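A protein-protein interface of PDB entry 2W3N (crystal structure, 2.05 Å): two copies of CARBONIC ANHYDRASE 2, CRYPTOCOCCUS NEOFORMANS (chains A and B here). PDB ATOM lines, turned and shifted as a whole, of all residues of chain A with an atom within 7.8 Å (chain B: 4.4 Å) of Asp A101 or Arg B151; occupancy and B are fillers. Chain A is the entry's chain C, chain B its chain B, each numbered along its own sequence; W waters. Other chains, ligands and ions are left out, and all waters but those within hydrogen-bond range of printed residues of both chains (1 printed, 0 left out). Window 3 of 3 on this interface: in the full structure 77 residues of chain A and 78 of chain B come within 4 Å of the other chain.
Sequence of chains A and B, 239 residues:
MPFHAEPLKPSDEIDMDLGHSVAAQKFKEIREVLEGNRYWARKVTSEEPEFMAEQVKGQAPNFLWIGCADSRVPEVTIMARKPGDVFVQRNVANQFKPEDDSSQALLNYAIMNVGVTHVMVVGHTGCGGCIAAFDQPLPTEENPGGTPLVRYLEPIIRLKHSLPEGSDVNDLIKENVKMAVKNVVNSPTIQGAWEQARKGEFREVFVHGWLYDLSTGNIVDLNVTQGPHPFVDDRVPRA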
ATOM      1  N   LYS A  97     -20.986  34.650  27.006  1.00  0.00           N
ATOM      2  CA  LYS A  97     -20.278  33.767  27.931  1.00  0.00           C
ATOM      3  C   LYS A  97     -18.952  33.389  27.326  1.00  0.00           C
ATOM      4  O   LYS A  97     -18.899  32.923  26.204  1.00  0.00           O
ATOM      5  CB  LYS A  97     -21.115  32.532  28.220  1.00  0.00           C
ATOM      6  CG  LYS A  97     -22.311  32.831  29.102  1.00  0.00           C
ATOM      7  CD  LYS A  97     -23.085  31.582  29.506  1.00  0.00           C
ATOM      8  CE  LYS A  97     -24.497  31.984  29.890  1.00  0.00           C
ATOM      9  NZ  LYS A  97     -25.100  31.320  31.098  1.00  0.00           N
ATOM     10  N   PRO A  98     -17.857  33.643  28.051  1.00  0.00           N
ATOM     11  CA  PRO A  98     -16.507  33.433  27.511  1.00  0.00           C
ATOM     12  C   PRO A  98     -16.162  31.955  27.233  1.00  0.00           C
ATOM     13  O   PRO A  98     -15.181  31.659  26.553  1.00  0.00           O
ATOM     14  CB  PRO A  98     -15.594  33.969  28.624  1.00  0.00           C
ATOM     15  CG  PRO A  98     -16.484  34.777  29.538  1.00  0.00           C
ATOM     16  CD  PRO A  98     -17.836  34.155  29.435  1.00  0.00           C
ATOM     17  N   GLU A  99     -16.949  31.025  27.746  1.00  0.00           N
ATOM     18  CA  GLU A  99     -16.606  29.624  27.541  1.00  0.00           C
ATOM     19  C   GLU A  99     -17.422  28.905  26.442  1.00  0.00           C
ATOM     20  O   GLU A  99     -17.144  27.743  26.134  1.00  0.00           O
ATOM     21  CB  GLU A  99     -16.640  28.867  28.877  1.00  0.00           C
ATOM     22  CG  GLU A  99     -18.018  28.447  29.328  1.00  0.00           C
ATOM     23  CD  GLU A  99     -18.831  29.573  29.937  1.00  0.00           C
ATOM     24  OE1 GLU A  99     -18.382  30.751  29.895  1.00  0.00           O
ATOM     25  OE2 GLU A  99     -19.929  29.268  30.454  1.00  0.00           O
ATOM     26  N   ASP A 100     -18.400  29.609  25.851  1.00  0.00           N
ATOM     27  CA  ASP A 100     -19.224  29.097  24.743  1.00  0.00           C
ATOM     28  C   ASP A 100     -18.543  29.137  23.395  1.00  0.00           C
ATOM     29  O   ASP A 100     -18.192  30.221  22.915  1.00  0.00           O
ATOM     30  CB  ASP A 100     -20.502  29.928  24.611  1.00  0.00           C
ATOM     31  CG  ASP A 100     -21.478  29.682  25.735  1.00  0.00           C
ATOM     32  OD1 ASP A 100     -21.012  29.485  26.880  1.00  0.00           O
ATOM     33  OD2 ASP A 100     -22.710  29.683  25.477  1.00  0.00           O
ATOM     34  N   ASP A 101     -18.413  27.986  22.736  1.00  0.00           N
ATOM     35  CA  ASP A 101     -17.877  27.982  21.371  1.00  0.00           C
ATOM     36  C   ASP A 101     -18.759  28.769  20.390  1.00  0.00           C
ATOM     37  O   ASP A 101     -18.265  29.336  19.409  1.00  0.00           O
ATOM     38  CB  ASP A 101     -17.685  26.557  20.838  1.00  0.00           C
ATOM     39  CG  ASP A 101     -16.540  25.822  21.519  1.00  0.00           C
ATOM     40  OD1 ASP A 101     -15.396  26.356  21.522  1.00  0.00           O
ATOM     41  OD2 ASP A 101     -16.798  24.711  22.050  1.00  0.00           O
ATOM     42  N   SER A 102     -20.060  28.784  20.649  1.00  0.00           N
ATOM     43  CA  SER A 102     -21.015  29.419  19.728  1.00  0.00           C
ATOM     44  C   SER A 102     -20.794  30.940  19.663  1.00  0.00           C
ATOM     45  O   SER A 102     -20.647  31.511  18.587  1.00  0.00           O
ATOM     46  CB  SER A 102     -22.449  29.079  20.138  1.00  0.00           C
ATOM     47  OG  SER A 102     -22.709  29.513  21.454  1.00  0.00           O
ATOM     48  N   SER A 103     -20.735  31.568  20.829  1.00  0.00           N
ATOM     49  CA  SER A 103     -20.445  32.998  20.931  1.00  0.00           C
ATOM     50  C   SER A 103     -19.043  33.311  20.443  1.00  0.00           C
ATOM     51  O   SER A 103     -18.829  34.263  19.677  1.00  0.00           O
ATOM     52  CB  SER A 103     -20.636  33.482  22.358  1.00  0.00           C
ATOM     53  OG  SER A 103     -22.000  33.392  22.698  1.00  0.00           O
ATOM     54  N   GLN A 104     -18.086  32.491  20.854  1.00  0.00           N
ATOM     55  CA  GLN A 104     -16.701  32.718  20.459  1.00  0.00           C
ATOM     56  C   GLN A 104     -16.493  32.519  18.955  1.00  0.00           C
ATOM     57  O   GLN A 104     -15.783  33.289  18.305  1.00  0.00           O
ATOM     58  CB  GLN A 104     -15.772  31.842  21.305  1.00  0.00           C
ATOM     59  CG  GLN A 104     -15.927  32.100  22.823  1.00  0.00           C
ATOM     60  CD  GLN A 104     -15.112  33.306  23.271  1.00  0.00           C
ATOM     61  OE1 GLN A 104     -14.427  33.933  22.463  1.00  0.00           O
ATOM     62  NE2 GLN A 104     -15.188  33.636  24.552  1.00  0.00           N
ATOM     63  N   ALA A 105     -17.132  31.507  18.385  1.00  0.00           N
ATOM     64  CA  ALA A 105     -17.093  31.311  16.923  1.00  0.00           C
ATOM     65  C   ALA A 105     -17.777  32.460  16.188  1.00  0.00           C
ATOM     66  O   ALA A 105     -17.311  32.937  15.157  1.00  0.00           O
ATOM     67  CB  ALA A 105     -17.769  30.027  16.579  1.00  0.00           C
ATOM     68  N   LEU A 106     -18.902  32.917  16.723  1.00  0.00           N
ATOM     69  CA  LEU A 106     -19.621  33.983  16.059  1.00  0.00           C
ATOM     70  C   LEU A 106     -18.728  35.217  16.061  1.00  0.00           C
ATOM     71  O   LEU A 106     -18.539  35.853  15.026  1.00  0.00           O
ATOM     72  CB  LEU A 106     -20.985  34.237  16.723  1.00  0.00           C
ATOM     73  CG  LEU A 106     -21.856  35.272  15.998  1.00  0.00           C
ATOM     74  CD1 LEU A 106     -23.359  35.015  16.216  1.00  0.00           C
ATOM     75  CD2 LEU A 106     -21.472  36.708  16.411  1.00  0.00           C
ATOM     76  N   LEU A 107     -18.154  35.535  17.213  1.00  0.00           N
ATOM     77  CA  LEU A 107     -17.359  36.770  17.333  1.00  0.00           C
ATOM     78  C   LEU A 107     -16.188  36.718  16.378  1.00  0.00           C
ATOM     79  O   LEU A 107     -15.904  37.669  15.656  1.00  0.00           O
ATOM     80  CB  LEU A 107     -16.884  36.989  18.768  1.00  0.00           C
ATOM     81  CG  LEU A 107     -15.949  38.176  19.041  1.00  0.00           C
ATOM     82  CD1 LEU A 107     -16.675  39.528  18.837  1.00  0.00           C
ATOM     83  CD2 LEU A 107     -15.450  38.063  20.444  1.00  0.00           C
ATOM     84  N   ASN A 108     -15.540  35.570  16.333  1.00  0.00           N
ATOM     85  CA  ASN A 108     -14.343  35.414  15.537  1.00  0.00           C
ATOM     86  C   ASN A 108     -14.642  35.452  14.062  1.00  0.00           C
ATOM     87  O   ASN A 108     -13.900  36.039  13.269  1.00  0.00           O
ATOM     88  CB  ASN A 108     -13.659  34.100  15.889  1.00  0.00           C
ATOM     89  CG  ASN A 108     -12.202  34.113  15.541  1.00  0.00           C
ATOM     90  OD1 ASN A 108     -11.819  33.760  14.419  1.00  0.00           O
ATOM     91  ND2 ASN A 108     -11.374  34.572  16.483  1.00  0.00           N
ATOM     92  N   LYS B  97     -29.376  23.516  19.120  1.00  0.00           N
ATOM     93  CA  LYS B  97     -28.768  22.291  19.628  1.00  0.00           C
ATOM     94  C   LYS B  97     -29.500  21.855  20.875  1.00  0.00           C
ATOM     95  O   LYS B  97     -29.669  22.651  21.807  1.00  0.00           O
ATOM     96  CB  LYS B  97     -27.292  22.523  19.968  1.00  0.00           C
ATOM     97  CG  LYS B  97     -26.519  23.247  18.915  1.00  0.00           C
ATOM     98  CD  LYS B  97     -24.983  23.096  19.120  1.00  0.00           C
ATOM     99  CE  LYS B  97     -24.248  23.489  17.812  1.00  0.00           C
ATOM    100  NZ  LYS B  97     -22.779  23.260  17.821  1.00  0.00           N
ATOM    101  N   GLY B 145     -11.731  18.389  16.432  1.00  0.00           N
ATOM    102  CA  GLY B 145     -12.283  19.654  15.954  1.00  0.00           C
ATOM    103  C   GLY B 145     -11.332  20.829  16.119  1.00  0.00           C
ATOM    104  O   GLY B 145     -11.122  21.304  17.239  1.00  0.00           O
ATOM    105  N   GLY B 146     -10.769  21.293  14.997  1.00  0.00           N
ATOM    106  CA  GLY B 146      -9.813  22.414  14.968  1.00  0.00           C
ATOM    107  C   GLY B 146     -10.178  23.614  15.842  1.00  0.00           C
ATOM    108  O   GLY B 146      -9.770  23.693  17.014  1.00  0.00           O
ATOM    109  N   THR B 147     -10.969  24.533  15.278  1.00  0.00           N
ATOM    110  CA  THR B 147     -11.332  25.808  15.923  1.00  0.00           C
ATOM    111  C   THR B 147     -12.656  25.734  16.725  1.00  0.00           C
ATOM    112  O   THR B 147     -13.329  24.700  16.726  1.00  0.00           O
ATOM    113  CB  THR B 147     -11.324  26.960  14.866  1.00  0.00           C
ATOM    114  OG1 THR B 147     -12.074  28.082  15.346  1.00  0.00           O
ATOM    115  CG2 THR B 147     -11.873  26.506  13.516  1.00  0.00           C
ATOM    116  N   PRO B 148     -13.016  26.809  17.455  1.00  0.00           N
ATOM    117  CA  PRO B 148     -14.413  26.920  17.949  1.00  0.00           C
ATOM    118  C   PRO B 148     -15.506  26.773  16.866  1.00  0.00           C
ATOM    119  O   PRO B 148     -16.546  26.164  17.134  1.00  0.00           O
ATOM    120  CB  PRO B 148     -14.461  28.320  18.583  1.00  0.00           C
ATOM    121  CG  PRO B 148     -13.040  28.588  18.994  1.00  0.00           C
ATOM    122  CD  PRO B 148     -12.178  27.934  17.915  1.00  0.00           C
ATOM    123  N   LEU B 149     -15.256  27.318  15.672  1.00  0.00           N
ATOM    124  CA  LEU B 149     -16.148  27.176  14.515  1.00  0.00           C
ATOM    125  C   LEU B 149     -16.396  25.718  14.058  1.00  0.00           C
ATOM    126  O   LEU B 149     -17.548  25.268  14.012  1.00  0.00           O
ATOM    127  CB  LEU B 149     -15.658  28.030  13.334  1.00  0.00           C
ATOM    128  CG  LEU B 149     -16.482  27.947  12.034  1.00  0.00           C
ATOM    129  CD1 LEU B 149     -17.834  28.643  12.173  1.00  0.00           C
ATOM    130  CD2 LEU B 149     -15.713  28.490  10.818  1.00  0.00           C
ATOM    131  N   VAL B 150     -15.325  25.001  13.701  1.00  0.00           N
ATOM    132  CA  VAL B 150     -15.436  23.614  13.241  1.00  0.00           C
ATOM    133  C   VAL B 150     -16.149  22.744  14.271  1.00  0.00           C
ATOM    134  O   VAL B 150     -17.013  21.933  13.930  1.00  0.00           O
ATOM    135  CB  VAL B 150     -14.054  23.023  12.896  1.00  0.00           C
ATOM    136  CG1 VAL B 150     -14.198  21.631  12.255  1.00  0.00           C
ATOM    137  CG2 VAL B 150     -13.318  23.958  11.957  1.00  0.00           C
ATOM    138  N   ARG B 151     -15.823  22.951  15.538  1.00  0.00           N
ATOM    139  CA  ARG B 151     -16.547  22.303  16.618  1.00  0.00           C
ATOM    140  C   ARG B 151     -18.018  22.720  16.699  1.00  0.00           C
ATOM    141  O   ARG B 151     -18.922  21.875  16.837  1.00  0.00           O
ATOM    142  CB  ARG B 151     -15.824  22.545  17.945  1.00  0.00           C
ATOM    143  CG  ARG B 151     -14.434  21.851  17.988  1.00  0.00           C
ATOM    144  CD  ARG B 151     -13.811  21.843  19.385  1.00  0.00           C
ATOM    145  NE  ARG B 151     -13.738  23.167  20.015  1.00  0.00           N
ATOM    146  CZ  ARG B 151     -12.647  23.937  20.048  1.00  0.00           C
ATOM    147  NH1 ARG B 151     -11.512  23.543  19.461  1.00  0.00           N
ATOM    148  NH2 ARG B 151     -12.696  25.108  20.667  1.00  0.00           N
ATOM    149  N   TYR B 152     -18.265  24.026  16.614  1.00  0.00           N
ATOM    150  CA  TYR B 152     -19.635  24.515  16.648  1.00  0.00           C
ATOM    151  C   TYR B 152     -20.416  23.931  15.468  1.00  0.00           C
ATOM    152  O   TYR B 152     -21.594  23.641  15.579  1.00  0.00           O
ATOM    153  CB  TYR B 152     -19.651  26.055  16.629  1.00  0.00           C
ATOM    154  CG  TYR B 152     -21.004  26.658  16.389  1.00  0.00           C
ATOM    155  CD1 TYR B 152     -21.944  26.762  17.407  1.00  0.00           C
ATOM    156  CD2 TYR B 152     -21.341  27.135  15.141  1.00  0.00           C
ATOM    157  CE1 TYR B 152     -23.228  27.326  17.166  1.00  0.00           C
ATOM    158  CE2 TYR B 152     -22.595  27.702  14.900  1.00  0.00           C
ATOM    159  CZ  TYR B 152     -23.511  27.794  15.906  1.00  0.00           C
ATOM    160  OH  TYR B 152     -24.723  28.363  15.607  1.00  0.00           O
ATOM    161  N   LEU B 153     -19.740  23.738  14.350  1.00  0.00           N
ATOM    162  CA  LEU B 153     -20.398  23.339  13.115  1.00  0.00           C
ATOM    163  C   LEU B 153     -20.548  21.819  12.997  1.00  0.00           C
ATOM    164  O   LEU B 153     -21.146  21.324  12.027  1.00  0.00           O
ATOM    165  CB  LEU B 153     -19.646  23.877  11.898  1.00  0.00           C
ATOM    166  CG  LEU B 153     -19.748  25.396  11.700  1.00  0.00           C
ATOM    167  CD1 LEU B 153     -19.023  25.739  10.415  1.00  0.00           C
ATOM    168  CD2 LEU B 153     -21.214  25.837  11.627  1.00  0.00           C
ATOM    169  N   GLU B 154     -20.029  21.094  13.983  1.00  0.00           N
ATOM    170  CA  GLU B 154     -20.062  19.621  13.939  1.00  0.00           C
ATOM    171  C   GLU B 154     -21.398  19.011  13.412  1.00  0.00           C
ATOM    172  O   GLU B 154     -21.358  18.172  12.501  1.00  0.00           O
ATOM    173  CB  GLU B 154     -19.716  19.022  15.307  1.00  0.00           C
ATOM    174  CG  GLU B 154     -19.844  17.495  15.362  1.00  0.00           C
ATOM    175  CD  GLU B 154     -19.376  16.918  16.713  1.00  0.00           C
ATOM    176  OE1 GLU B 154     -19.986  15.926  17.203  1.00  0.00           O
ATOM    177  OE2 GLU B 154     -18.398  17.474  17.281  1.00  0.00           O
HETATM  178  O   HOH W   1     -23.152  31.041  16.744  1.00  0.00           O
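Water W1 bridges O of Ser A102 and OH of Tyr B152.
Position printed for both chains: 97.
The guanidinium group of Arg B151 is in salt-bridge range of the side-chain carboxylate of Asp A101, at 3.1 Å.
Of the 11 printed residues of chain B, 4 touch a printed residue of chain A. Printed residues of chain B that touch a printed residue of chain A: Pro B148, Leu B149, Arg B151 and Tyr B152. Hydrophobic or aromatic side chains of chain B that line the printed part of chain A: Pro B148 and Tyr B152. Along chain B the printed residues that touch a printed residue of chain A span positions 148 to 152. Among the printed residues, Asp or Glu carboxylates within 4 Å of a Lys or Arg side-chain nitrogen of the other chain: Asp A101 with Arg B151 (3.1 Å).
The side-chain amino group (NZ) of Lys B97 lies within hydrogen-bond range of the backbone carbonyl oxygen (O) of Tyr B152, at 2.6 Å. The guanidinium group (NH1) of Arg B151 lies within hydrogen-bond range of the backbone carbonyl oxygen (O) of Gly B145, 3.2 Å away. The backbone carbonyl oxygen (O) of Gly B146 is in hydrogen-bond range of the guanidinium group (NH1) of Arg B151 (3.0 Å). The side-chain hydroxyl of Thr B147 lies close to the backbone NH of Leu B149, at 3.3 Å. The backbone carbonyl oxygen (O) of Thr B147 lies close to the guanidinium group (NH1) of Arg B151.
Among the printed residues, merely in contact across the chains: Ser A102 with Tyr B152, Asp A101 with Pro B148, Ala A105 with Leu B149 and Ala A105 with Pro B148.
Of chain B, only Pro B148 and Arg B151 come within 4 Å of Asp A101. Arg B151 touches one residue of chain A. Printed residues of chain B within 4 Å of Ser A102: Tyr B152. Of the printed residues of chain A, Leu B149 touches Ala A105. Printed residues of chain A within 4 Å of Tyr B152: Ser A102 (3.5 Å). Val B150 touches none of the printed residues of chain A. Asp A100 touches none of the printed residues of chain B. The nearest residue of chain A that does not touch Arg B151 is Ala A105 (7.3 Å).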
